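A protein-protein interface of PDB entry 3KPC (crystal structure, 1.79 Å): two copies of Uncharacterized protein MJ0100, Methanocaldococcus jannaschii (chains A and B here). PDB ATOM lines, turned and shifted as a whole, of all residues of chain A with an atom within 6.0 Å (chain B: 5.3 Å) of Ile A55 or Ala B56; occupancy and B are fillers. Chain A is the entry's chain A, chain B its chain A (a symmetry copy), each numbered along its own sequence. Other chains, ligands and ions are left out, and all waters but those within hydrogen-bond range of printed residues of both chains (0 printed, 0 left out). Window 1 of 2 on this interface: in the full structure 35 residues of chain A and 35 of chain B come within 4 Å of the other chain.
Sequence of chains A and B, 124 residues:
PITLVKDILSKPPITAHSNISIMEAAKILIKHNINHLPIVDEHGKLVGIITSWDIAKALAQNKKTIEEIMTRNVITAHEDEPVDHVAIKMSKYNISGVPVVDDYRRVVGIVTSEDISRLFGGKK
Of the 10 printed residues of chain B, 8 touch a printed residue of chain A.
Printed residues of chain B that touch a printed residue of chain A: Ser B52, Trp B53, Ile B55, Ala B56, Lys B57, Leu B59, Ala B60 and Gln B61.
Hydrophobic or aromatic side chains of chain B within 4 Å of the printed part of chain A: Trp B53, Ile B55, Ala B56, Leu B59 and Ala B60.
Hydrophobic or aromatic side chains of chain A that line the printed part of chain B: Ile A22, Ala A26, Ile A30, Trp A53, Ile A55, Ala A56 and Leu A59.
Among the printed residues, no Asp or Glu carboxylate lies within 4 Å of a Lys or Arg side-chain nitrogen of the other chain.
Ser B52 touches its own counterpart, Ser A52.
Ser A52 touches Trp B53, and with the chains exchanged Trp A53 touches Ser B52.
Ile A55 touches Ala B56, and with the chains exchanged Ala A56 touches Ile B55.
Ile A55 touches Leu B59, and with the chains exchanged Leu A59 touches Ile B55.
OG1 of Thr A51 sits close to N of Trp A53 (3.3 Å).
NZ of Lys B57 sits close to NE2 of Gln B61.
Among the printed residues, merely in contact across the chains: Ile A22 with Leu B59, Ala A26 with Ala B56, Ala A26 with Ala B60, Lys A27 with Ala B60, Ile A30 with Trp B53, Ile A30 with Lys B57, Ile A30 with Ala B60, Ile A30 with Gln B61, Ser A52 with Ser B52, Ser A52 with Trp B53, Trp A53 with Ser B52, Ile A55 with Ala B56, Ile A55 with Leu B59, Ala A56 with Ile B55 and Leu A59 with Ile B55.
The backbone carbonyl oxygen (O) of Leu A29 sits at hydrogen-bond distance from the indole nitrogen (NE1) of Trp B53, 3.3 Å away.
Ile A55 touches just these residues of chain B: Ala B56 and Leu B59.
Ala B56 touches just these residues of chain A: Ala A26 and Ile A55.
Of the printed residues of chain A, Trp B53 touches Leu A29 (3.3 Å), Ile A30 (3.5 Å) and Ser A52 (3.7 Å).
Printed residues of chain B within 4 Å of Trp A53: Ser B52.
Of the printed residues of chain A, Gln B61 touches Ile A30 (3.7 Å).
The nearest residue of chain B that does not touch Ile A55 is Ile B55 (4.9 Å).
The nearest residue of chain A that does not touch Ala B56 is Ile A30 (4.2 Å).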
ATOM      1  N   ILE A  22       2.563  14.865  14.407  1.00  0.00           N
ATOM      2  CA  ILE A  22       1.933  13.948  13.455  1.00  0.00           C
ATOM      3  C   ILE A  22       1.300  12.756  14.186  1.00  0.00           C
ATOM      4  O   ILE A  22       0.181  12.353  13.853  1.00  0.00           O
ATOM      5  CB  ILE A  22       2.908  13.490  12.340  1.00  0.00           C
ATOM      6  CG1 ILE A  22       3.376  14.706  11.530  1.00  0.00           C
ATOM      7  CG2 ILE A  22       2.248  12.457  11.422  1.00  0.00           C
ATOM      8  CD1 ILE A  22       4.376  14.398  10.430  1.00  0.00           C
ATOM      9  N   ALA A  25      -1.952  13.907  15.767  1.00  0.00           N
ATOM     10  CA  ALA A  25      -2.990  14.009  14.739  1.00  0.00           C
ATOM     11  C   ALA A  25      -3.565  12.634  14.408  1.00  0.00           C
ATOM     12  O   ALA A  25      -4.784  12.475  14.324  1.00  0.00           O
ATOM     13  CB  ALA A  25      -2.449  14.677  13.487  1.00  0.00           C
ATOM     14  N   ALA A  26      -2.683  11.651  14.228  1.00  0.00           N
ATOM     15  CA  ALA A  26      -3.098  10.275  13.956  1.00  0.00           C
ATOM     16  C   ALA A  26      -4.008   9.753  15.067  1.00  0.00           C
ATOM     17  O   ALA A  26      -5.030   9.121  14.790  1.00  0.00           O
ATOM     18  CB  ALA A  26      -1.883   9.371  13.784  1.00  0.00           C
ATOM     19  N   LYS A  27      -3.636  10.039  16.315  1.00  0.00           N
ATOM     20  CA  LYS A  27      -4.415   9.629  17.486  1.00  0.00           C
ATOM     21  C   LYS A  27      -5.835  10.206  17.480  1.00  0.00           C
ATOM     22  O   LYS A  27      -6.782   9.523  17.873  1.00  0.00           O
ATOM     23  CB  LYS A  27      -3.681   9.994  18.784  1.00  0.00           C
ATOM     24  CG  LYS A  27      -2.503   9.077  19.128  1.00  0.00           C
ATOM     25  CD  LYS A  27      -1.708   9.600  20.321  1.00  0.00           C
ATOM     26  CE  LYS A  27      -0.606   8.627  20.742  1.00  0.00           C
ATOM     27  NZ  LYS A  27       0.170   9.147  21.917  1.00  0.00           N
ATOM     28  N   LEU A  29      -7.570  11.081  14.725  1.00  0.00           N
ATOM     29  CA  LEU A  29      -8.276  10.360  13.661  1.00  0.00           C
ATOM     30  C   LEU A  29      -8.797   9.004  14.130  1.00  0.00           C
ATOM     31  O   LEU A  29      -9.921   8.617  13.796  1.00  0.00           O
ATOM     32  CB  LEU A  29      -7.386  10.181  12.421  1.00  0.00           C
ATOM     33  CG  LEU A  29      -6.893  11.429  11.677  1.00  0.00           C
ATOM     34  CD1 LEU A  29      -5.990  11.026  10.517  1.00  0.00           C
ATOM     35  CD2 LEU A  29      -8.043  12.306  11.179  1.00  0.00           C
ATOM     36  N   ILE A  30      -7.983   8.295  14.909  1.00  0.00           N
ATOM     37  CA  ILE A  30      -8.375   6.988  15.434  1.00  0.00           C
ATOM     38  C   ILE A  30      -9.435   7.119  16.533  1.00  0.00           C
ATOM     39  O   ILE A  30     -10.441   6.406  16.510  1.00  0.00           O
ATOM     40  CB  ILE A  30      -7.156   6.158  15.928  1.00  0.00           C
ATOM     41  CG1 ILE A  30      -6.088   5.998  14.829  1.00  0.00           C
ATOM     42  CG2 ILE A  30      -7.587   4.802  16.509  1.00  0.00           C
ATOM     43  CD1 ILE A  30      -6.623   5.671  13.430  1.00  0.00           C
ATOM     44  N   ILE A  50      -5.624  18.194   7.364  1.00  0.00           N
ATOM     45  CA  ILE A  50      -4.874  16.949   7.443  1.00  0.00           C
ATOM     46  C   ILE A  50      -5.848  15.802   7.212  1.00  0.00           C
ATOM     47  O   ILE A  50      -6.942  15.793   7.781  1.00  0.00           O
ATOM     48  CB  ILE A  50      -4.229  16.795   8.850  1.00  0.00           C
ATOM     49  CG1 ILE A  50      -3.040  17.749   9.019  1.00  0.00           C
ATOM     50  CG2 ILE A  50      -3.848  15.333   9.159  1.00  0.00           C
ATOM     51  CD1 ILE A  50      -1.796  17.363   8.237  1.00  0.00           C
ATOM     52  N   THR A  51      -5.470  14.845   6.371  1.00  0.00           N
ATOM     53  CA  THR A  51      -6.268  13.633   6.219  1.00  0.00           C
ATOM     54  C   THR A  51      -5.399  12.420   6.517  1.00  0.00           C
ATOM     55  O   THR A  51      -4.175  12.553   6.655  1.00  0.00           O
ATOM     56  CB  THR A  51      -6.893  13.509   4.809  1.00  0.00           C
ATOM     57  OG1 THR A  51      -5.878  13.221   3.841  1.00  0.00           O
ATOM     58  CG2 THR A  51      -7.641  14.780   4.411  1.00  0.00           C
ATOM     59  N   SER A  52      -6.023  11.247   6.617  1.00  0.00           N
ATOM     60  CA  SER A  52      -5.295   9.991   6.812  1.00  0.00           C
ATOM     61  C   SER A  52      -4.232   9.790   5.732  1.00  0.00           C
ATOM     62  O   SER A  52      -3.162   9.239   5.993  1.00  0.00           O
ATOM     63  CB  SER A  52      -6.262   8.802   6.817  1.00  0.00           C
ATOM     64  OG  SER A  52      -7.202   8.907   7.873  1.00  0.00           O
ATOM     65  N   TRP A  53      -4.543  10.228   4.513  1.00  0.00           N
ATOM     66  CA  TRP A  53      -3.620  10.118   3.380  1.00  0.00           C
ATOM     67  C   TRP A  53      -2.330  10.907   3.627  1.00  0.00           C
ATOM     68  O   TRP A  53      -1.241  10.460   3.253  1.00  0.00           O
ATOM     69  CB  TRP A  53      -4.308  10.602   2.109  1.00  0.00           C
ATOM     70  CG  TRP A  53      -3.603  10.263   0.839  1.00  0.00           C
ATOM     71  CD1 TRP A  53      -3.723   9.111   0.114  1.00  0.00           C
ATOM     72  CD2 TRP A  53      -2.694  11.102   0.114  1.00  0.00           C
ATOM     73  NE1 TRP A  53      -2.933   9.173  -1.010  1.00  0.00           N
ATOM     74  CE2 TRP A  53      -2.294  10.386  -1.039  1.00  0.00           C
ATOM     75  CE3 TRP A  53      -2.173  12.387   0.329  1.00  0.00           C
ATOM     76  CZ2 TRP A  53      -1.390  10.912  -1.975  1.00  0.00           C
ATOM     77  CZ3 TRP A  53      -1.276  12.912  -0.605  1.00  0.00           C
ATOM     78  CH2 TRP A  53      -0.894  12.171  -1.741  1.00  0.00           C
ATOM     79  N   ASP A  54      -2.458  12.073   4.263  1.00  0.00           N
ATOM     80  CA  ASP A  54      -1.293  12.872   4.650  1.00  0.00           C
ATOM     81  C   ASP A  54      -0.448  12.192   5.722  1.00  0.00           C
ATOM     82  O   ASP A  54       0.779  12.313   5.704  1.00  0.00           O
ATOM     83  CB  ASP A  54      -1.706  14.263   5.134  1.00  0.00           C
ATOM     84  CG  ASP A  54      -2.381  15.080   4.052  1.00  0.00           C
ATOM     85  OD1 ASP A  54      -1.856  15.131   2.918  1.00  0.00           O
ATOM     86  OD2 ASP A  54      -3.433  15.683   4.342  1.00  0.00           O
ATOM     87  N   ILE A  55      -1.097  11.495   6.656  1.00  0.00           N
ATOM     88  CA  ILE A  55      -0.374  10.731   7.677  1.00  0.00           C
ATOM     89  C   ILE A  55       0.413   9.608   6.995  1.00  0.00           C
ATOM     90  O   ILE A  55       1.577   9.370   7.329  1.00  0.00           O
ATOM     91  CB  ILE A  55      -1.322  10.160   8.776  1.00  0.00           C
ATOM     92  CG1 ILE A  55      -2.183  11.268   9.408  1.00  0.00           C
ATOM     93  CG2 ILE A  55      -0.533   9.381   9.841  1.00  0.00           C
ATOM     94  CD1 ILE A  55      -1.413  12.355  10.170  1.00  0.00           C
ATOM     95  N   ALA A  56      -0.221   8.939   6.029  1.00  0.00           N
ATOM     96  CA  ALA A  56       0.455   7.924   5.220  1.00  0.00           C
ATOM     97  C   ALA A  56       1.627   8.523   4.437  1.00  0.00           C
ATOM     98  O   ALA A  56       2.693   7.903   4.345  1.00  0.00           O
ATOM     99  CB  ALA A  56      -0.529   7.230   4.283  1.00  0.00           C
ATOM    100  N   LYS A  57       1.439   9.725   3.890  1.00  0.00           N
ATOM    101  CA  LYS A  57       2.498  10.428   3.146  1.00  0.00           C
ATOM    102  C   LYS A  57       3.703  10.753   4.030  1.00  0.00           C
ATOM    103  O   LYS A  57       4.852  10.666   3.582  1.00  0.00           O
ATOM    104  CB  LYS A  57       1.958  11.708   2.487  1.00  0.00           C
ATOM    105  CG  LYS A  57       2.898  12.366   1.466  1.00  0.00           C
ATOM    106  CD  LYS A  57       2.212  13.536   0.762  1.00  0.00           C
ATOM    107  CE  LYS A  57       3.034  14.064  -0.416  1.00  0.00           C
ATOM    108  NZ  LYS A  57       3.975  15.151  -0.022  1.00  0.00           N
ATOM    109  N   ALA A  58       3.434  11.119   5.285  1.00  0.00           N
ATOM    110  CA  ALA A  58       4.491  11.428   6.244  1.00  0.00           C
ATOM    111  C   ALA A  58       5.398  10.219   6.452  1.00  0.00           C
ATOM    112  O   ALA A  58       6.621  10.358   6.509  1.00  0.00           O
ATOM    113  CB  ALA A  58       3.895  11.890   7.568  1.00  0.00           C
ATOM    114  N   LEU A  59       4.787   9.039   6.558  1.00  0.00           N
ATOM    115  CA  LEU A  59       5.534   7.792   6.697  1.00  0.00           C
ATOM    116  C   LEU A  59       6.298   7.464   5.413  1.00  0.00           C
ATOM    117  O   LEU A  59       7.484   7.128   5.464  1.00  0.00           O
ATOM    118  CB  LEU A  59       4.607   6.630   7.080  1.00  0.00           C
ATOM    119  CG  LEU A  59       5.276   5.262   7.277  1.00  0.00           C
ATOM    120  CD1 LEU A  59       6.199   5.239   8.505  1.00  0.00           C
ATOM    121  CD2 LEU A  59       4.235   4.156   7.385  1.00  0.00           C
ATOM    122  N   ALA A  60       5.610   7.565   4.274  1.00  0.00           N
ATOM    123  CA  ALA A  60       6.195   7.236   2.972  1.00  0.00           C
ATOM    124  C   ALA A  60       7.394   8.110   2.602  1.00  0.00           C
ATOM    125  O   ALA A  60       8.333   7.639   1.954  1.00  0.00           O
ATOM    126  CB  ALA A  60       5.133   7.306   1.883  1.00  0.00           C
ATOM    127  N   ILE A  66       3.149  18.553  11.060  1.00  0.00           N
ATOM    128  CA  ILE A  66       1.824  18.880  10.538  1.00  0.00           C
ATOM    129  C   ILE A  66       1.882  20.080   9.586  1.00  0.00           C
ATOM    130  O   ILE A  66       1.269  20.054   8.516  1.00  0.00           O
ATOM    131  CB  ILE A  66       0.810  19.131  11.697  1.00  0.00           C
ATOM    132  CG1 ILE A  66       0.491  17.820  12.440  1.00  0.00           C
ATOM    133  CG2 ILE A  66      -0.473  19.819  11.198  1.00  0.00           C
ATOM    134  CD1 ILE A  66      -0.099  16.697  11.575  1.00  0.00           C
ATOM    135  N   ILE A  69       3.080  19.019   6.189  1.00  0.00           N
ATOM    136  CA  ILE A  69       2.255  18.093   5.411  1.00  0.00           C
ATOM    137  C   ILE A  69       0.813  18.532   5.165  1.00  0.00           C
ATOM    138  O   ILE A  69       0.151  17.981   4.281  1.00  0.00           O
ATOM    139  CB  ILE A  69       2.260  16.648   6.001  1.00  0.00           C
ATOM    140  CG1 ILE A  69       1.599  16.605   7.389  1.00  0.00           C
ATOM    141  CG2 ILE A  69       3.679  16.114   6.056  1.00  0.00           C
ATOM    142  CD1 ILE A  69       1.271  15.183   7.874  1.00  0.00           C
ATOM    143  N   SER B  52      -5.689   4.140   4.294  1.00  0.00           N
ATOM    144  CA  SER B  52      -4.886   5.208   4.893  1.00  0.00           C
ATOM    145  C   SER B  52      -5.129   5.307   6.399  1.00  0.00           C
ATOM    146  O   SER B  52      -4.216   5.616   7.167  1.00  0.00           O
ATOM    147  CB  SER B  52      -5.194   6.553   4.227  1.00  0.00           C
ATOM    148  OG  SER B  52      -4.885   6.525   2.844  1.00  0.00           O
ATOM    149  N   TRP B  53      -6.371   5.060   6.813  1.00  0.00           N
ATOM    150  CA  TRP B  53      -6.750   5.104   8.227  1.00  0.00           C
ATOM    151  C   TRP B  53      -5.983   4.062   9.048  1.00  0.00           C
ATOM    152  O   TRP B  53      -5.592   4.328  10.189  1.00  0.00           O
ATOM    153  CB  TRP B  53      -8.253   4.889   8.361  1.00  0.00           C
ATOM    154  CG  TRP B  53      -8.822   5.211   9.703  1.00  0.00           C
ATOM    155  CD1 TRP B  53      -9.254   6.431  10.140  1.00  0.00           C
ATOM    156  CD2 TRP B  53      -9.061   4.290  10.775  1.00  0.00           C
ATOM    157  NE1 TRP B  53      -9.735   6.330  11.425  1.00  0.00           N
ATOM    158  CE2 TRP B  53      -9.633   5.027  11.839  1.00  0.00           C
ATOM    159  CE3 TRP B  53      -8.843   2.913  10.944  1.00  0.00           C
ATOM    160  CZ2 TRP B  53      -9.986   4.434  13.060  1.00  0.00           C
ATOM    161  CZ3 TRP B  53      -9.198   2.323  12.158  1.00  0.00           C
ATOM    162  CH2 TRP B  53      -9.762   3.086  13.200  1.00  0.00           C
ATOM    163  N   ASP B  54      -5.762   2.886   8.459  1.00  0.00           N
ATOM    164  CA  ASP B  54      -4.953   1.844   9.098  1.00  0.00           C
ATOM    165  C   ASP B  54      -3.486   2.240   9.225  1.00  0.00           C
ATOM    166  O   ASP B  54      -2.840   1.889  10.215  1.00  0.00           O
ATOM    167  CB  ASP B  54      -5.058   0.516   8.344  1.00  0.00           C
ATOM    168  CG  ASP B  54      -6.465  -0.045   8.346  1.00  0.00           C
ATOM    169  OD1 ASP B  54      -7.099  -0.084   9.424  1.00  0.00           O
ATOM    170  OD2 ASP B  54      -6.932  -0.461   7.268  1.00  0.00           O
ATOM    171  N   ILE B  55      -2.960   2.953   8.227  1.00  0.00           N
ATOM    172  CA  ILE B  55      -1.586   3.459   8.294  1.00  0.00           C
ATOM    173  C   ILE B  55      -1.484   4.473   9.438  1.00  0.00           C
ATOM    174  O   ILE B  55      -0.520   4.450  10.208  1.00  0.00           O
ATOM    175  CB  ILE B  55      -1.117   4.089   6.947  1.00  0.00           C
ATOM    176  CG1 ILE B  55      -1.298   3.107   5.775  1.00  0.00           C
ATOM    177  CG2 ILE B  55       0.332   4.593   7.042  1.00  0.00           C
ATOM    178  CD1 ILE B  55      -0.461   1.824   5.846  1.00  0.00           C
ATOM    179  N   ALA B  56      -2.490   5.343   9.553  1.00  0.00           N
ATOM    180  CA  ALA B  56      -2.573   6.286  10.669  1.00  0.00           C
ATOM    181  C   ALA B  56      -2.667   5.555  12.012  1.00  0.00           C
ATOM    182  O   ALA B  56      -2.029   5.966  12.987  1.00  0.00           O
ATOM    183  CB  ALA B  56      -3.746   7.244  10.487  1.00  0.00           C
ATOM    184  N   LYS B  57      -3.444   4.471  12.058  1.00  0.00           N
ATOM    185  CA  LYS B  57      -3.589   3.655  13.276  1.00  0.00           C
ATOM    186  C   LYS B  57      -2.266   3.019  13.705  1.00  0.00           C
ATOM    187  O   LYS B  57      -1.970   2.930  14.901  1.00  0.00           O
ATOM    188  CB  LYS B  57      -4.667   2.574  13.095  1.00  0.00           C
ATOM    189  CG  LYS B  57      -5.094   1.853  14.383  1.00  0.00           C
ATOM    190  CD  LYS B  57      -6.269   0.911  14.121  1.00  0.00           C
ATOM    191  CE  LYS B  57      -6.864   0.355  15.417  1.00  0.00           C
ATOM    192  NZ  LYS B  57      -6.228  -0.925  15.841  1.00  0.00           N
ATOM    193  N   ALA B  58      -1.471   2.590  12.722  1.00  0.00           N
ATOM    194  CA  ALA B  58      -0.166   1.991  12.988  1.00  0.00           C
ATOM    195  C   ALA B  58       0.738   2.977  13.720  1.00  0.00           C
ATOM    196  O   ALA B  58       1.439   2.603  14.661  1.00  0.00           O
ATOM    197  CB  ALA B  58       0.483   1.522  11.692  1.00  0.00           C
ATOM    198  N   LEU B  59       0.709   4.236  13.281  1.00  0.00           N
ATOM    199  CA  LEU B  59       1.476   5.298  13.928  1.00  0.00           C
ATOM    200  C   LEU B  59       0.927   5.600  15.324  1.00  0.00           C
ATOM    201  O   LEU B  59       1.693   5.696  16.286  1.00  0.00           O
ATOM    202  CB  LEU B  59       1.491   6.572  13.072  1.00  0.00           C
ATOM    203  CG  LEU B  59       2.284   7.760  13.634  1.00  0.00           C
ATOM    204  CD1 LEU B  59       3.795   7.485  13.669  1.00  0.00           C
ATOM    205  CD2 LEU B  59       2.002   9.029  12.839  1.00  0.00           C
ATOM    206  N   ALA B  60      -0.397   5.745  15.420  1.00  0.00           N
ATOM    207  CA  ALA B  60      -1.060   6.084  16.681  1.00  0.00           C
ATOM    208  C   ALA B  60      -0.858   5.037  17.778  1.00  0.00           C
ATOM    209  O   ALA B  60      -0.768   5.383  18.960  1.00  0.00           O
ATOM    210  CB  ALA B  60      -2.545   6.327  16.448  1.00  0.00           C
ATOM    211  N   GLN B  61      -0.774   3.769  17.385  1.00  0.00           N
ATOM    212  CA  GLN B  61      -0.795   2.675  18.354  1.00  0.00           C
ATOM    213  C   GLN B  61       0.440   1.778  18.326  1.00  0.00           C
ATOM    214  O   GLN B  61       0.438   0.688  18.910  1.00  0.00           O
ATOM    215  CB  GLN B  61      -2.074   1.852  18.177  1.00  0.00           C
ATOM    216  CG  GLN B  61      -3.333   2.676  18.392  1.00  0.00           C
ATOM    217  CD  GLN B  61      -4.614   1.883  18.264  1.00  0.00           C
ATOM    218  OE1 GLN B  61      -5.692   2.383  18.584  1.00  0.00           O
ATOM    219  NE2 GLN B  61      -4.511   0.646  17.794  1.00  0.00           N
